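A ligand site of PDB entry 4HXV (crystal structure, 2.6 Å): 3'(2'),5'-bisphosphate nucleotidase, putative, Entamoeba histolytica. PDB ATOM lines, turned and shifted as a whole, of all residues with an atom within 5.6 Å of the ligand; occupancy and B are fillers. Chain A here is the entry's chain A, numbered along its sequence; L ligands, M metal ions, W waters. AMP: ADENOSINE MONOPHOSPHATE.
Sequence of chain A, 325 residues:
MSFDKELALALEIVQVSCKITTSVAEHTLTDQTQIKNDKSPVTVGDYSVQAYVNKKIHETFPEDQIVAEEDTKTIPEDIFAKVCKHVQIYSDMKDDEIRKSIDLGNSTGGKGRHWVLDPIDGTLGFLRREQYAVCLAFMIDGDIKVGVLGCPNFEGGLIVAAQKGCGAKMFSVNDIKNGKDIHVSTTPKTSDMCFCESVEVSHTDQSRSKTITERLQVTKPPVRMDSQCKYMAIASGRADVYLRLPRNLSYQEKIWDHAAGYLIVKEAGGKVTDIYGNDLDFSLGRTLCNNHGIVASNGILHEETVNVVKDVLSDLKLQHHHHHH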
ATOM      1  N   GLU A  69     -18.393 -29.342  -2.633  1.00  0.00           N
ATOM      2  CA  GLU A  69     -18.393 -28.438  -3.773  1.00  0.00           C
ATOM      3  C   GLU A  69     -17.701 -28.958  -5.036  1.00  0.00           C
ATOM      4  O   GLU A  69     -18.281 -28.895  -6.123  1.00  0.00           O
ATOM      5  CB  GLU A  69     -17.818 -27.075  -3.399  1.00  0.00           C
ATOM      6  CG  GLU A  69     -17.751 -26.109  -4.564  1.00  0.00           C
ATOM      7  CD  GLU A  69     -17.262 -24.738  -4.178  1.00  0.00           C
ATOM      8  OE1 GLU A  69     -16.697 -24.583  -3.071  1.00  0.00           O
ATOM      9  OE2 GLU A  69     -17.425 -23.813  -4.985  1.00  0.00           O
ATOM     10  N   ASP A 118     -17.332 -27.478   2.460  1.00  0.00           N
ATOM     11  CA  ASP A 118     -16.613 -26.547   1.611  1.00  0.00           C
ATOM     12  C   ASP A 118     -15.111 -26.670   1.855  1.00  0.00           C
ATOM     13  O   ASP A 118     -14.629 -26.279   2.902  1.00  0.00           O
ATOM     14  CB  ASP A 118     -17.057 -25.115   1.814  1.00  0.00           C
ATOM     15  CG  ASP A 118     -16.995 -24.318   0.536  1.00  0.00           C
ATOM     16  OD1 ASP A 118     -16.265 -24.731  -0.388  1.00  0.00           O
ATOM     17  OD2 ASP A 118     -17.698 -23.307   0.425  1.00  0.00           O
ATOM     18  N   ASP A 121     -13.732 -22.246   1.572  1.00  0.00           N
ATOM     19  CA  ASP A 121     -14.841 -21.344   1.449  1.00  0.00           C
ATOM     20  C   ASP A 121     -14.309 -19.941   1.266  1.00  0.00           C
ATOM     21  O   ASP A 121     -13.469 -19.484   2.038  1.00  0.00           O
ATOM     22  CB  ASP A 121     -15.671 -21.415   2.707  1.00  0.00           C
ATOM     23  CG  ASP A 121     -17.005 -20.836   2.515  1.00  0.00           C
ATOM     24  OD1 ASP A 121     -17.195 -19.633   2.805  1.00  0.00           O
ATOM     25  OD2 ASP A 121     -17.890 -21.567   2.028  1.00  0.00           O
ATOM     26  N   GLY A 122     -14.796 -19.267   0.226  1.00  0.00           N
ATOM     27  CA  GLY A 122     -14.217 -17.996  -0.204  1.00  0.00           C
ATOM     28  C   GLY A 122     -12.855 -18.211  -0.833  1.00  0.00           C
ATOM     29  O   GLY A 122     -11.849 -17.740  -0.319  1.00  0.00           O
ATOM     30  N   SER A 198     -19.794  -9.693   2.119  1.00  0.00           N
ATOM     31  CA  SER A 198     -18.795 -10.159   1.152  1.00  0.00           C
ATOM     32  C   SER A 198     -17.992  -9.024   0.530  1.00  0.00           C
ATOM     33  O   SER A 198     -18.444  -7.876   0.507  1.00  0.00           O
ATOM     34  CB  SER A 198     -19.471 -10.938   0.034  1.00  0.00           C
ATOM     35  OG  SER A 198     -20.343 -11.912   0.544  1.00  0.00           O
ATOM     36  N   VAL A 199     -16.812  -9.356   0.011  1.00  0.00           N
ATOM     37  CA  VAL A 199     -15.956  -8.381  -0.626  1.00  0.00           C
ATOM     38  C   VAL A 199     -16.379  -8.262  -2.072  1.00  0.00           C
ATOM     39  O   VAL A 199     -16.360  -7.174  -2.628  1.00  0.00           O
ATOM     40  CB  VAL A 199     -14.486  -8.804  -0.638  1.00  0.00           C
ATOM     41  CG1 VAL A 199     -13.687  -7.908  -1.559  1.00  0.00           C
ATOM     42  CG2 VAL A 199     -13.909  -8.773   0.775  1.00  0.00           C
ATOM     43  N   GLU A 200     -16.767  -9.385  -2.648  1.00  0.00           N
ATOM     44  CA  GLU A 200     -17.239  -9.436  -4.019  1.00  0.00           C
ATOM     45  C   GLU A 200     -18.585  -8.768  -4.264  1.00  0.00           C
ATOM     46  O   GLU A 200     -19.549  -8.978  -3.529  1.00  0.00           O
ATOM     47  CB  GLU A 200     -17.292 -10.880  -4.481  1.00  0.00           C
ATOM     48  CG  GLU A 200     -15.897 -11.448  -4.655  1.00  0.00           C
ATOM     49  CD  GLU A 200     -15.087 -10.684  -5.686  1.00  0.00           C
ATOM     50  OE1 GLU A 200     -15.470 -10.682  -6.884  1.00  0.00           O
ATOM     51  OE2 GLU A 200     -14.050 -10.097  -5.303  1.00  0.00           O
ATOM     52  N   SER A 202     -20.448  -9.346  -6.711  1.00  0.00           N
ATOM     53  CA  SER A 202     -21.381 -10.270  -7.333  1.00  0.00           C
ATOM     54  C   SER A 202     -22.055 -11.136  -6.286  1.00  0.00           C
ATOM     55  O   SER A 202     -23.088 -11.729  -6.542  1.00  0.00           O
ATOM     56  CB  SER A 202     -20.711 -11.127  -8.407  1.00  0.00           C
ATOM     57  OG  SER A 202     -19.408 -11.517  -8.027  1.00  0.00           O
ATOM     58  N   HIS A 203     -21.477 -11.172  -5.089  1.00  0.00           N
ATOM     59  CA  HIS A 203     -22.028 -12.022  -4.054  1.00  0.00           C
ATOM     60  C   HIS A 203     -22.965 -11.344  -3.115  1.00  0.00           C
ATOM     61  O   HIS A 203     -23.641 -12.033  -2.340  1.00  0.00           O
ATOM     62  CB  HIS A 203     -20.929 -12.684  -3.289  1.00  0.00           C
ATOM     63  CG  HIS A 203     -20.047 -13.534  -4.146  1.00  0.00           C
ATOM     64  ND1 HIS A 203     -18.870 -14.011  -3.719  1.00  0.00           N
ATOM     65  CD2 HIS A 203     -20.201 -13.980  -5.453  1.00  0.00           C
ATOM     66  CE1 HIS A 203     -18.298 -14.747  -4.695  1.00  0.00           C
ATOM     67  NE2 HIS A 203     -19.115 -14.734  -5.760  1.00  0.00           N
ATOM     68  N   THR A 204     -23.001 -10.017  -3.140  1.00  0.00           N
ATOM     69  CA  THR A 204     -23.921  -9.266  -2.293  1.00  0.00           C
ATOM     70  C   THR A 204     -24.132  -7.869  -2.820  1.00  0.00           C
ATOM     71  O   THR A 204     -23.255  -7.288  -3.442  1.00  0.00           O
ATOM     72  CB  THR A 204     -23.432  -9.178  -0.833  1.00  0.00           C
ATOM     73  OG1 THR A 204     -24.518  -8.747  -0.001  1.00  0.00           O
ATOM     74  CG2 THR A 204     -22.262  -8.213  -0.705  1.00  0.00           C
ATOM     75  N   MET A 225     -15.553  -8.740   4.008  1.00  0.00           N
ATOM     76  CA  MET A 225     -14.675  -9.892   4.136  1.00  0.00           C
ATOM     77  C   MET A 225     -15.225 -11.148   3.453  1.00  0.00           C
ATOM     78  O   MET A 225     -16.429 -11.310   3.279  1.00  0.00           O
ATOM     79  CB  MET A 225     -14.327 -10.170   5.595  1.00  0.00           C
ATOM     80  CG  MET A 225     -15.368 -10.993   6.339  1.00  0.00           C
ATOM     81  SD  MET A 225     -14.825 -11.502   7.974  1.00  0.00           S
ATOM     82  CE  MET A 225     -14.220 -13.123   7.554  1.00  0.00           C
ATOM     83  N   ASP A 226     -14.317 -12.035   3.082  1.00  0.00           N
ATOM     84  CA  ASP A 226     -14.697 -13.204   2.322  1.00  0.00           C
ATOM     85  C   ASP A 226     -14.992 -14.333   3.266  1.00  0.00           C
ATOM     86  O   ASP A 226     -14.498 -14.349   4.399  1.00  0.00           O
ATOM     87  CB  ASP A 226     -13.564 -13.640   1.415  1.00  0.00           C
ATOM     88  CG  ASP A 226     -13.178 -12.575   0.408  1.00  0.00           C
ATOM     89  OD1 ASP A 226     -13.847 -12.454  -0.646  1.00  0.00           O
ATOM     90  OD2 ASP A 226     -12.158 -11.888   0.640  1.00  0.00           O
ATOM     91  N   SER A 227     -15.830 -15.264   2.795  1.00  0.00           N
ATOM     92  CA  SER A 227     -16.028 -16.598   3.388  1.00  0.00           C
ATOM     93  C   SER A 227     -16.950 -16.688   4.612  1.00  0.00           C
ATOM     94  O   SER A 227     -17.374 -15.678   5.185  1.00  0.00           O
ATOM     95  CB  SER A 227     -14.685 -17.217   3.738  1.00  0.00           C
ATOM     96  OG  SER A 227     -14.247 -16.743   4.998  1.00  0.00           O
ATOM     97  N   GLN A 228     -17.250 -17.917   5.024  1.00  0.00           N
ATOM     98  CA  GLN A 228     -18.040 -18.136   6.219  1.00  0.00           C
ATOM     99  C   GLN A 228     -17.364 -17.591   7.466  1.00  0.00           C
ATOM    100  O   GLN A 228     -17.905 -17.711   8.545  1.00  0.00           O
ATOM    101  CB  GLN A 228     -18.337 -19.616   6.430  1.00  0.00           C
ATOM    102  CG  GLN A 228     -19.442 -20.157   5.542  1.00  0.00           C
ATOM    103  CD  GLN A 228     -20.077 -21.396   6.121  1.00  0.00           C
ATOM    104  OE1 GLN A 228     -20.882 -21.322   7.031  1.00  0.00           O
ATOM    105  NE2 GLN A 228     -19.718 -22.553   5.578  1.00  0.00           N
ATOM    106  N   LYS A 230     -17.454 -14.888   8.172  1.00  0.00           N
ATOM    107  CA  LYS A 230     -18.399 -13.846   8.570  1.00  0.00           C
ATOM    108  C   LYS A 230     -19.345 -14.334   9.642  1.00  0.00           C
ATOM    109  O   LYS A 230     -19.827 -13.541  10.455  1.00  0.00           O
ATOM    110  CB  LYS A 230     -19.167 -13.351   7.353  1.00  0.00           C
ATOM    111  CG  LYS A 230     -18.366 -12.397   6.488  1.00  0.00           C
ATOM    112  CD  LYS A 230     -19.233 -11.777   5.412  1.00  0.00           C
ATOM    113  CE  LYS A 230     -19.677 -12.805   4.394  1.00  0.00           C
ATOM    114  NZ  LYS A 230     -18.605 -13.124   3.419  1.00  0.00           N
ATOM    115  N   TYR A 242     -24.683  -9.580   9.929  1.00  0.00           N
ATOM    116  CA  TYR A 242     -24.067 -10.058   8.704  1.00  0.00           C
ATOM    117  C   TYR A 242     -25.154 -10.172   7.653  1.00  0.00           C
ATOM    118  O   TYR A 242     -26.113 -10.927   7.837  1.00  0.00           O
ATOM    119  CB  TYR A 242     -23.364 -11.402   8.954  1.00  0.00           C
ATOM    120  CG  TYR A 242     -23.168 -12.268   7.741  1.00  0.00           C
ATOM    121  CD1 TYR A 242     -22.847 -11.714   6.505  1.00  0.00           C
ATOM    122  CD2 TYR A 242     -23.301 -13.647   7.833  1.00  0.00           C
ATOM    123  CE1 TYR A 242     -22.694 -12.504   5.404  1.00  0.00           C
ATOM    124  CE2 TYR A 242     -23.124 -14.440   6.737  1.00  0.00           C
ATOM    125  CZ  TYR A 242     -22.819 -13.863   5.526  1.00  0.00           C
ATOM    126  OH  TYR A 242     -22.639 -14.643   4.425  1.00  0.00           O
ATOM    127  N   ARG A 244     -26.337 -10.791   3.579  1.00  0.00           N
ATOM    128  CA  ARG A 244     -26.008 -11.294   2.288  1.00  0.00           C
ATOM    129  C   ARG A 244     -27.249 -10.996   1.508  1.00  0.00           C
ATOM    130  O   ARG A 244     -28.297 -11.554   1.807  1.00  0.00           O
ATOM    131  CB  ARG A 244     -25.761 -12.775   2.368  1.00  0.00           C
ATOM    132  CG  ARG A 244     -24.923 -13.279   1.227  1.00  0.00           C
ATOM    133  CD  ARG A 244     -24.775 -14.779   1.325  1.00  0.00           C
ATOM    134  NE  ARG A 244     -24.031 -15.276   0.190  1.00  0.00           N
ATOM    135  CZ  ARG A 244     -22.705 -15.282   0.123  1.00  0.00           C
ATOM    136  NH1 ARG A 244     -21.982 -14.828   1.142  1.00  0.00           N
ATOM    137  NH2 ARG A 244     -22.098 -15.753  -0.952  1.00  0.00           N
ATOM    138  N   TYR A 251     -31.306 -16.882  -7.528  1.00  0.00           N
ATOM    139  CA  TYR A 251     -30.111 -17.462  -6.936  1.00  0.00           C
ATOM    140  C   TYR A 251     -30.507 -18.319  -5.740  1.00  0.00           C
ATOM    141  O   TYR A 251     -31.302 -17.897  -4.897  1.00  0.00           O
ATOM    142  CB  TYR A 251     -29.079 -16.405  -6.532  1.00  0.00           C
ATOM    143  CG  TYR A 251     -27.852 -17.052  -5.986  1.00  0.00           C
ATOM    144  CD1 TYR A 251     -27.591 -17.025  -4.628  1.00  0.00           C
ATOM    145  CD2 TYR A 251     -26.996 -17.753  -6.824  1.00  0.00           C
ATOM    146  CE1 TYR A 251     -26.486 -17.649  -4.122  1.00  0.00           C
ATOM    147  CE2 TYR A 251     -25.891 -18.377  -6.318  1.00  0.00           C
ATOM    148  CZ  TYR A 251     -25.645 -18.311  -4.969  1.00  0.00           C
ATOM    149  OH  TYR A 251     -24.557 -18.930  -4.461  1.00  0.00           O
ATOM    150  N   GLU A 253     -28.748 -20.133  -2.596  1.00  0.00           N
ATOM    151  CA  GLU A 253     -27.530 -20.372  -1.836  1.00  0.00           C
ATOM    152  C   GLU A 253     -27.177 -21.852  -1.633  1.00  0.00           C
ATOM    153  O   GLU A 253     -28.031 -22.683  -1.322  1.00  0.00           O
ATOM    154  CB  GLU A 253     -27.639 -19.674  -0.499  1.00  0.00           C
ATOM    155  CG  GLU A 253     -27.688 -18.155  -0.614  1.00  0.00           C
ATOM    156  CD  GLU A 253     -26.317 -17.526  -0.779  1.00  0.00           C
ATOM    157  OE1 GLU A 253     -25.281 -18.239  -0.744  1.00  0.00           O
ATOM    158  OE2 GLU A 253     -26.258 -16.294  -0.949  1.00  0.00           O
ATOM    159  N   LYS A 254     -25.893 -22.150  -1.805  1.00  0.00           N
ATOM    160  CA  LYS A 254     -25.378 -23.499  -1.567  1.00  0.00           C
ATOM    161  C   LYS A 254     -25.385 -23.798  -0.076  1.00  0.00           C
ATOM    162  O   LYS A 254     -25.117 -22.928   0.755  1.00  0.00           O
ATOM    163  CB  LYS A 254     -23.953 -23.659  -2.114  1.00  0.00           C
ATOM    164  CG  LYS A 254     -23.783 -23.490  -3.623  1.00  0.00           C
ATOM    165  CD  LYS A 254     -25.063 -23.805  -4.374  1.00  0.00           C
ATOM    166  CE  LYS A 254     -25.011 -23.385  -5.839  1.00  0.00           C
ATOM    167  NZ  LYS A 254     -25.615 -22.041  -6.129  1.00  0.00           N
ATOM    168  N   TRP A 256     -23.267 -25.546   1.423  1.00  0.00           N
ATOM    169  CA  TRP A 256     -21.902 -25.563   1.923  1.00  0.00           C
ATOM    170  C   TRP A 256     -21.358 -24.184   2.093  1.00  0.00           C
ATOM    171  O   TRP A 256     -20.231 -23.992   2.538  1.00  0.00           O
ATOM    172  CB  TRP A 256     -20.983 -26.411   1.071  1.00  0.00           C
ATOM    173  CG  TRP A 256     -21.024 -26.063  -0.368  1.00  0.00           C
ATOM    174  CD1 TRP A 256     -20.353 -25.039  -1.004  1.00  0.00           C
ATOM    175  CD2 TRP A 256     -21.772 -26.730  -1.398  1.00  0.00           C
ATOM    176  NE1 TRP A 256     -20.633 -25.034  -2.335  1.00  0.00           N
ATOM    177  CE2 TRP A 256     -21.478 -26.023  -2.642  1.00  0.00           C
ATOM    178  CE3 TRP A 256     -22.613 -27.801  -1.415  1.00  0.00           C
ATOM    179  CZ2 TRP A 256     -22.026 -26.407  -3.841  1.00  0.00           C
ATOM    180  CZ3 TRP A 256     -23.171 -28.175  -2.634  1.00  0.00           C
ATOM    181  CH2 TRP A 256     -22.884 -27.491  -3.809  1.00  0.00           C
ATOM    182  N   ASP A 257     -22.168 -23.195   1.779  1.00  0.00           N
ATOM    183  CA  ASP A 257     -21.817 -21.860   2.125  1.00  0.00           C
ATOM    184  C   ASP A 257     -22.387 -21.420   3.444  1.00  0.00           C
ATOM    185  O   ASP A 257     -22.061 -20.337   3.905  1.00  0.00           O
ATOM    186  CB  ASP A 257     -22.296 -20.909   1.053  1.00  0.00           C
ATOM    187  CG  ASP A 257     -21.397 -20.898  -0.129  1.00  0.00           C
ATOM    188  OD1 ASP A 257     -20.198 -21.221   0.022  1.00  0.00           O
ATOM    189  OD2 ASP A 257     -21.877 -20.580  -1.234  1.00  0.00           O
HETATM  190  P   AMP L   1     -18.081 -14.636  -0.143  1.00  0.00           P
HETATM  191  O1P AMP L   1     -18.965 -14.171   0.996  1.00  0.00           O
HETATM  192  O2P AMP L   1     -16.793 -15.287   0.285  1.00  0.00           O
HETATM  193  O3P AMP L   1     -17.922 -13.612  -1.242  1.00  0.00           O
HETATM  194  O5' AMP L   1     -18.932 -15.817  -0.786  1.00  0.00           O
HETATM  195  C5' AMP L   1     -18.295 -16.877  -1.505  1.00  0.00           C
HETATM  196  C4' AMP L   1     -19.414 -17.785  -1.972  1.00  0.00           C
HETATM  197  O4' AMP L   1     -20.423 -17.019  -2.623  1.00  0.00           O
HETATM  198  C3' AMP L   1     -18.972 -18.836  -2.971  1.00  0.00           C
HETATM  199  O3' AMP L   1     -18.813 -20.090  -2.295  1.00  0.00           O
HETATM  200  C2' AMP L   1     -20.102 -18.916  -3.987  1.00  0.00           C
HETATM  201  O2' AMP L   1     -20.698 -20.214  -4.038  1.00  0.00           O
HETATM  202  C1' AMP L   1     -21.120 -17.916  -3.490  1.00  0.00           C
HETATM  203  N9  AMP L   1     -21.799 -17.216  -4.617  1.00  0.00           N
HETATM  204  C8  AMP L   1     -21.527 -17.350  -5.925  1.00  0.00           C
HETATM  205  N7  AMP L   1     -22.351 -16.575  -6.678  1.00  0.00           N
HETATM  206  C5  AMP L   1     -23.179 -15.928  -5.841  1.00  0.00           C
HETATM  207  C6  AMP L   1     -24.296 -14.963  -5.970  1.00  0.00           C
HETATM  208  N6  AMP L   1     -24.699 -14.513  -7.185  1.00  0.00           N
HETATM  209  N1  AMP L   1     -24.902 -14.533  -4.829  1.00  0.00           N
HETATM  210  C2  AMP L   1     -24.515 -14.979  -3.613  1.00  0.00           C
HETATM  211  N3  AMP L   1     -23.504 -15.862  -3.426  1.00  0.00           N
HETATM  212  C4  AMP L   1     -22.812 -16.358  -4.479  1.00  0.00           C
HETATM  213 MG    MG M   1     -15.029 -22.981  -2.373  1.00  0.00          MG
HETATM  214  O   HOH W   1     -15.661 -20.342  -2.978  1.00  0.00           O
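Gly 122 touches the ligand (CA to O2P, 3.8 Å).
Asp 226 touches the ligand (CA to O2P, 3.6 Å).
Glu 253 touches the ligand.
Hydrophobic or aromatic side chains that line the ligand: His 203 and Tyr 251.
Within 4 Å of the ligand: Gly 122, Ser 198, Ser 202, His 203, Asp 226, Ser 227, Lys 230, Arg 244, Tyr 251, Glu 253 and Asp 257.
The nearest printed residue that does not touch the ligand is Glu 200 (4.3 Å).
The side-chain hydroxyl (OG) of Ser 198 lies within hydrogen-bond range of an oxygen (O1P) of the ligand, at 2.7 Å.
N6 of the ligand sits at hydrogen-bond distance from O of Ser 202 (3.3 Å).
A nitrogen (N3) of the ligand lies close to the side-chain hydroxyl (OH) of Tyr 251 (3.4 Å).
An oxygen (O1P) of the ligand lies within salt-bridge range of the guanidinium group (NH1) of Arg 244, 3.1 Å away.
The side-chain amino group (NZ) of Lys 230 lies within salt-bridge range of an oxygen (O1P) of the ligand, at 2.7 Å.
OD1 of Asp 257 sits at hydrogen-bond distance from O3' of the ligand, at 2.9 Å.
O3P of the ligand sits at hydrogen-bond distance from ND1 of His 203, 2.7 Å away.
The backbone NH (N) of Ser 227 lies within hydrogen-bond range of an oxygen (O2P) of the ligand (2.7 Å).
Water W1 bridges an oxygen (O3') of the ligand (3.2 Å) and the backbone NH (N) of Gly 122 (3.5 Å).
The guanidinium group of Arg 244 is in salt-bridge range of the side-chain carboxylate of Glu 253 (2.7 Å).
O of Ser 227 is in hydrogen-bond range of NZ of Lys 230 (3.3 Å).
The side-chain amide oxygen of Gln 228 lies close to the backbone carbonyl oxygen of Asp 257 (3.5 Å).
The guanidinium group (NH1) of Arg 244 lies within hydrogen-bond range of the side-chain hydroxyl (OH) of Tyr 242 (3.4 Å).
The side-chain amino group of Lys 230 is in hydrogen-bond range of the backbone carbonyl oxygen of Met 225.
The guanidinium group (NH1) of Arg 244 sits at hydrogen-bond distance from the side-chain hydroxyl (OG) of Ser 198 (3.4 Å).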
